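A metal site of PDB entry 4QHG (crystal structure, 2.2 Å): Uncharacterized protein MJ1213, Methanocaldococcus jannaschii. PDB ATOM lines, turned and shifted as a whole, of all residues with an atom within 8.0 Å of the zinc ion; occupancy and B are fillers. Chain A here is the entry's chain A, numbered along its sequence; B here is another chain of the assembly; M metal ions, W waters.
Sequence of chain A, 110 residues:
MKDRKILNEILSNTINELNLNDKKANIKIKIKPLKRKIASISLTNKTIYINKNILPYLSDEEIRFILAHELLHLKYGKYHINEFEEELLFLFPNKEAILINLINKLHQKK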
ATOM      1  N   ALA A  39       2.732 -15.695  30.715  1.00  0.00           N
ATOM      2  CA  ALA A  39       2.897 -16.243  29.379  1.00  0.00           C
ATOM      3  C   ALA A  39       2.635 -15.191  28.343  1.00  0.00           C
ATOM      4  O   ALA A  39       1.959 -14.202  28.604  1.00  0.00           O
ATOM      5  CB  ALA A  39       1.943 -17.423  29.172  1.00  0.00           C
ATOM      6  N   SER A  40       3.182 -15.418  27.170  1.00  0.00           N
ATOM      7  CA  SER A  40       3.030 -14.524  26.041  1.00  0.00           C
ATOM      8  C   SER A  40       3.176 -15.326  24.786  1.00  0.00           C
ATOM      9  O   SER A  40       3.621 -16.469  24.837  1.00  0.00           O
ATOM     10  CB  SER A  40       4.070 -13.413  26.114  1.00  0.00           C
ATOM     11  OG  SER A  40       3.755 -12.397  25.176  1.00  0.00           O
ATOM     12  N   ILE A  41       2.792 -14.743  23.638  1.00  0.00           N
ATOM     13  CA  ILE A  41       2.932 -15.404  22.357  1.00  0.00           C
ATOM     14  C   ILE A  41       3.319 -14.396  21.297  1.00  0.00           C
ATOM     15  O   ILE A  41       2.817 -13.272  21.282  1.00  0.00           O
ATOM     16  CB  ILE A  41       1.670 -16.218  21.932  1.00  0.00           C
ATOM     17  CG1 ILE A  41       1.963 -17.075  20.647  1.00  0.00           C
ATOM     18  CG2 ILE A  41       0.394 -15.318  21.810  1.00  0.00           C
ATOM     19  CD1 ILE A  41       0.880 -18.140  20.208  1.00  0.00           C
ATOM     20  N   PHE A  65      -4.169 -24.848  30.609  1.00  0.00           N
ATOM     21  CA  PHE A  65      -4.980 -23.643  30.492  1.00  0.00           C
ATOM     22  C   PHE A  65      -4.178 -22.511  29.797  1.00  0.00           C
ATOM     23  O   PHE A  65      -4.676 -21.915  28.857  1.00  0.00           O
ATOM     24  CB  PHE A  65      -5.519 -23.167  31.869  1.00  0.00           C
ATOM     25  CG  PHE A  65      -6.223 -21.838  31.778  1.00  0.00           C
ATOM     26  CD1 PHE A  65      -7.490 -21.736  31.205  1.00  0.00           C
ATOM     27  CD2 PHE A  65      -5.596 -20.667  32.203  1.00  0.00           C
ATOM     28  CE1 PHE A  65      -8.114 -20.501  31.060  1.00  0.00           C
ATOM     29  CE2 PHE A  65      -6.210 -19.424  32.040  1.00  0.00           C
ATOM     30  CZ  PHE A  65      -7.475 -19.357  31.479  1.00  0.00           C
ATOM     31  N   ILE A  66      -2.938 -22.263  30.256  1.00  0.00           N
ATOM     32  CA  ILE A  66      -2.039 -21.236  29.735  1.00  0.00           C
ATOM     33  C   ILE A  66      -1.729 -21.478  28.234  1.00  0.00           C
ATOM     34  O   ILE A  66      -1.759 -20.531  27.451  1.00  0.00           O
ATOM     35  CB  ILE A  66      -0.756 -21.202  30.604  1.00  0.00           C
ATOM     36  CG1 ILE A  66      -1.020 -20.398  31.903  1.00  0.00           C
ATOM     37  CG2 ILE A  66       0.451 -20.642  29.847  1.00  0.00           C
ATOM     38  CD1 ILE A  66      -0.126 -20.725  33.091  1.00  0.00           C
ATOM     39  N   LEU A  67      -1.451 -22.731  27.831  1.00  0.00           N
ATOM     40  CA  LEU A  67      -1.134 -23.067  26.447  1.00  0.00           C
ATOM     41  C   LEU A  67      -2.357 -22.899  25.546  1.00  0.00           C
ATOM     42  O   LEU A  67      -2.207 -22.346  24.459  1.00  0.00           O
ATOM     43  CB  LEU A  67      -0.537 -24.477  26.311  1.00  0.00           C
ATOM     44  CG  LEU A  67       0.854 -24.688  26.915  1.00  0.00           C
ATOM     45  CD1 LEU A  67       1.324 -26.125  26.709  1.00  0.00           C
ATOM     46  CD2 LEU A  67       1.874 -23.681  26.388  1.00  0.00           C
ATOM     47  N   ALA A  68      -3.564 -23.332  26.017  1.00  0.00           N
ATOM     48  CA  ALA A  68      -4.808 -23.151  25.254  1.00  0.00           C
ATOM     49  C   ALA A  68      -5.142 -21.668  25.075  1.00  0.00           C
ATOM     50  O   ALA A  68      -5.569 -21.279  23.991  1.00  0.00           O
ATOM     51  CB  ALA A  68      -5.964 -23.888  25.930  1.00  0.00           C
ATOM     52  N   HIS A  69      -4.906 -20.839  26.112  1.00  0.00           N
ATOM     53  CA  HIS A  69      -5.163 -19.399  26.053  1.00  0.00           C
ATOM     54  C   HIS A  69      -4.284 -18.709  25.022  1.00  0.00           C
ATOM     55  O   HIS A  69      -4.760 -17.826  24.297  1.00  0.00           O
ATOM     56  CB  HIS A  69      -4.963 -18.724  27.443  1.00  0.00           C
ATOM     57  CG  HIS A  69      -5.548 -17.346  27.504  1.00  0.00           C
ATOM     58  ND1 HIS A  69      -4.897 -16.249  26.927  1.00  0.00           N
ATOM     59  CD2 HIS A  69      -6.738 -16.929  27.998  1.00  0.00           C
ATOM     60  CE1 HIS A  69      -5.711 -15.219  27.106  1.00  0.00           C
ATOM     61  NE2 HIS A  69      -6.839 -15.583  27.739  1.00  0.00           N
ATOM     62  N   GLU A  70      -3.009 -19.093  24.949  1.00  0.00           N
ATOM     63  CA  GLU A  70      -2.064 -18.471  24.031  1.00  0.00           C
ATOM     64  C   GLU A  70      -2.257 -18.938  22.603  1.00  0.00           C
ATOM     65  O   GLU A  70      -2.204 -18.113  21.687  1.00  0.00           O
ATOM     66  CB  GLU A  70      -0.632 -18.708  24.519  1.00  0.00           C
ATOM     67  CG  GLU A  70      -0.347 -17.947  25.815  1.00  0.00           C
ATOM     68  CD  GLU A  70      -0.944 -16.554  25.865  1.00  0.00           C
ATOM     69  OE1 GLU A  70      -0.319 -15.629  25.299  1.00  0.00           O
ATOM     70  OE2 GLU A  70      -2.079 -16.404  26.377  1.00  0.00           O
ATOM     71  N   LEU A  71      -2.535 -20.228  22.407  1.00  0.00           N
ATOM     72  CA  LEU A  71      -2.765 -20.799  21.076  1.00  0.00           C
ATOM     73  C   LEU A  71      -4.060 -20.271  20.458  1.00  0.00           C
ATOM     74  O   LEU A  71      -4.138 -20.146  19.251  1.00  0.00           O
ATOM     75  CB  LEU A  71      -2.789 -22.331  21.120  1.00  0.00           C
ATOM     76  CG  LEU A  71      -1.440 -23.038  21.291  1.00  0.00           C
ATOM     77  CD1 LEU A  71      -1.631 -24.514  21.548  1.00  0.00           C
ATOM     78  CD2 LEU A  71      -0.540 -22.849  20.065  1.00  0.00           C
ATOM     79  N   LEU A  72      -5.072 -19.930  21.292  1.00  0.00           N
ATOM     80  CA  LEU A  72      -6.347 -19.387  20.799  1.00  0.00           C
ATOM     81  C   LEU A  72      -6.182 -17.989  20.155  1.00  0.00           C
ATOM     82  O   LEU A  72      -7.061 -17.580  19.387  1.00  0.00           O
ATOM     83  CB  LEU A  72      -7.432 -19.373  21.900  1.00  0.00           C
ATOM     84  CG  LEU A  72      -8.264 -20.654  22.063  1.00  0.00           C
ATOM     85  CD1 LEU A  72      -9.076 -20.610  23.347  1.00  0.00           C
ATOM     86  CD2 LEU A  72      -9.172 -20.915  20.825  1.00  0.00           C
ATOM     87  N   HIS A  73      -5.058 -17.275  20.414  1.00  0.00           N
ATOM     88  CA  HIS A  73      -4.753 -15.988  19.754  1.00  0.00           C
ATOM     89  C   HIS A  73      -4.395 -16.201  18.284  1.00  0.00           C
ATOM     90  O   HIS A  73      -4.390 -15.246  17.508  1.00  0.00           O
ATOM     91  CB  HIS A  73      -3.609 -15.237  20.455  1.00  0.00           C
ATOM     92  CG  HIS A  73      -3.940 -14.887  21.865  1.00  0.00           C
ATOM     93  ND1 HIS A  73      -5.080 -14.179  22.178  1.00  0.00           N
ATOM     94  CD2 HIS A  73      -3.274 -15.170  23.004  1.00  0.00           C
ATOM     95  CE1 HIS A  73      -5.084 -14.075  23.490  1.00  0.00           C
ATOM     96  NE2 HIS A  73      -4.038 -14.681  24.022  1.00  0.00           N
ATOM     97  N   PHE A  84     -13.559 -16.615  20.893  1.00  0.00           N
ATOM     98  CA  PHE A  84     -12.363 -16.913  21.701  1.00  0.00           C
ATOM     99  C   PHE A  84     -12.772 -17.473  23.080  1.00  0.00           C
ATOM    100  O   PHE A  84     -12.307 -18.538  23.469  1.00  0.00           O
ATOM    101  CB  PHE A  84     -11.489 -15.656  21.875  1.00  0.00           C
ATOM    102  CG  PHE A  84     -10.226 -15.856  22.689  1.00  0.00           C
ATOM    103  CD1 PHE A  84     -10.263 -15.883  24.081  1.00  0.00           C
ATOM    104  CD2 PHE A  84      -8.984 -15.964  22.063  1.00  0.00           C
ATOM    105  CE1 PHE A  84      -9.096 -16.092  24.825  1.00  0.00           C
ATOM    106  CE2 PHE A  84      -7.816 -16.137  22.819  1.00  0.00           C
ATOM    107  CZ  PHE A  84      -7.876 -16.205  24.190  1.00  0.00           C
ATOM    108  N   LEU A  88     -12.512 -21.218  24.850  1.00  0.00           N
ATOM    109  CA  LEU A  88     -11.767 -21.295  26.103  1.00  0.00           C
ATOM    110  C   LEU A  88     -12.655 -21.858  27.227  1.00  0.00           C
ATOM    111  O   LEU A  88     -12.206 -22.747  27.956  1.00  0.00           O
ATOM    112  CB  LEU A  88     -11.228 -19.913  26.498  1.00  0.00           C
ATOM    113  CG  LEU A  88     -10.277 -19.867  27.693  1.00  0.00           C
ATOM    114  CD1 LEU A  88      -8.960 -20.600  27.403  1.00  0.00           C
ATOM    115  CD2 LEU A  88     -10.014 -18.428  28.090  1.00  0.00           C
ATOM    116  N   ASN B 104      -6.043 -10.211  33.650  1.00  0.00           N
ATOM    117  CA  ASN B 104      -6.428  -9.993  32.258  1.00  0.00           C
ATOM    118  C   ASN B 104      -5.768  -8.729  31.710  1.00  0.00           C
ATOM    119  O   ASN B 104      -5.154  -8.795  30.657  1.00  0.00           O
ATOM    120  CB  ASN B 104      -7.948  -9.886  32.104  1.00  0.00           C
ATOM    121  CG  ASN B 104      -8.740 -11.170  32.283  1.00  0.00           C
ATOM    122  OD1 ASN B 104      -8.218 -12.240  32.602  1.00  0.00           O
ATOM    123  ND2 ASN B 104     -10.044 -11.068  32.101  1.00  0.00           N
ATOM    124  N   HIS B 107      -2.043  -9.055  31.258  1.00  0.00           N
ATOM    125  CA  HIS B 107      -1.796  -9.989  30.161  1.00  0.00           C
ATOM    126  C   HIS B 107      -1.975  -9.347  28.780  1.00  0.00           C
ATOM    127  O   HIS B 107      -1.237  -9.701  27.849  1.00  0.00           O
ATOM    128  CB  HIS B 107      -2.721 -11.208  30.277  1.00  0.00           C
ATOM    129  CG  HIS B 107      -2.345 -12.304  29.323  1.00  0.00           C
ATOM    130  ND1 HIS B 107      -1.077 -12.844  29.324  1.00  0.00           N
ATOM    131  CD2 HIS B 107      -3.089 -12.922  28.392  1.00  0.00           C
ATOM    132  CE1 HIS B 107      -1.086 -13.777  28.392  1.00  0.00           C
ATOM    133  NE2 HIS B 107      -2.277 -13.883  27.821  1.00  0.00           N
ATOM    134  N   GLN B 108      -2.950  -8.439  28.637  1.00  0.00           N
ATOM    135  CA  GLN B 108      -3.241  -7.752  27.369  1.00  0.00           C
ATOM    136  C   GLN B 108      -2.325  -6.564  27.139  1.00  0.00           C
ATOM    137  O   GLN B 108      -1.959  -6.294  25.988  1.00  0.00           O
ATOM    138  CB  GLN B 108      -4.694  -7.283  27.339  1.00  0.00           C
ATOM    139  CG  GLN B 108      -5.646  -8.299  26.759  1.00  0.00           C
ATOM    140  CD  GLN B 108      -6.669  -8.720  27.766  1.00  0.00           C
ATOM    141  OE1 GLN B 108      -7.678  -8.035  27.977  1.00  0.00           O
ATOM    142  NE2 GLN B 108      -6.441  -9.858  28.396  1.00  0.00           N
HETATM  143 ZN    ZN M   1      -3.262 -14.871  26.043  1.00  0.00          ZN
HETATM  144  O   HOH W   1      -3.279 -12.877  25.584  1.00  0.00           O
HETATM  145  O   HOH W   2      -0.737 -13.048  24.682  1.00  0.00           O
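Along chain A the residues within 4 Å of the zinc ion span positions 69 to 73.
The nearest printed residue that does not touch the zinc ion is Phe 84 (5.1 Å).
The zinc ion is bound by the side-chain carboxylate of Glu 70 (2.0 Å), water W1 (2.0 Å), a ring nitrogen (NE2) of His 73 (2.2 Å), a ring nitrogen (NE2) of His 107 of chain B (2.3 Å) and a ring nitrogen (ND1) of His 69 (2.3 Å).
The zinc ion has five donor atoms within binding distance.
A ring nitrogen (ND1) of His 107 of chain B sits close to the backbone carbonyl oxygen (O) of Ala 39.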
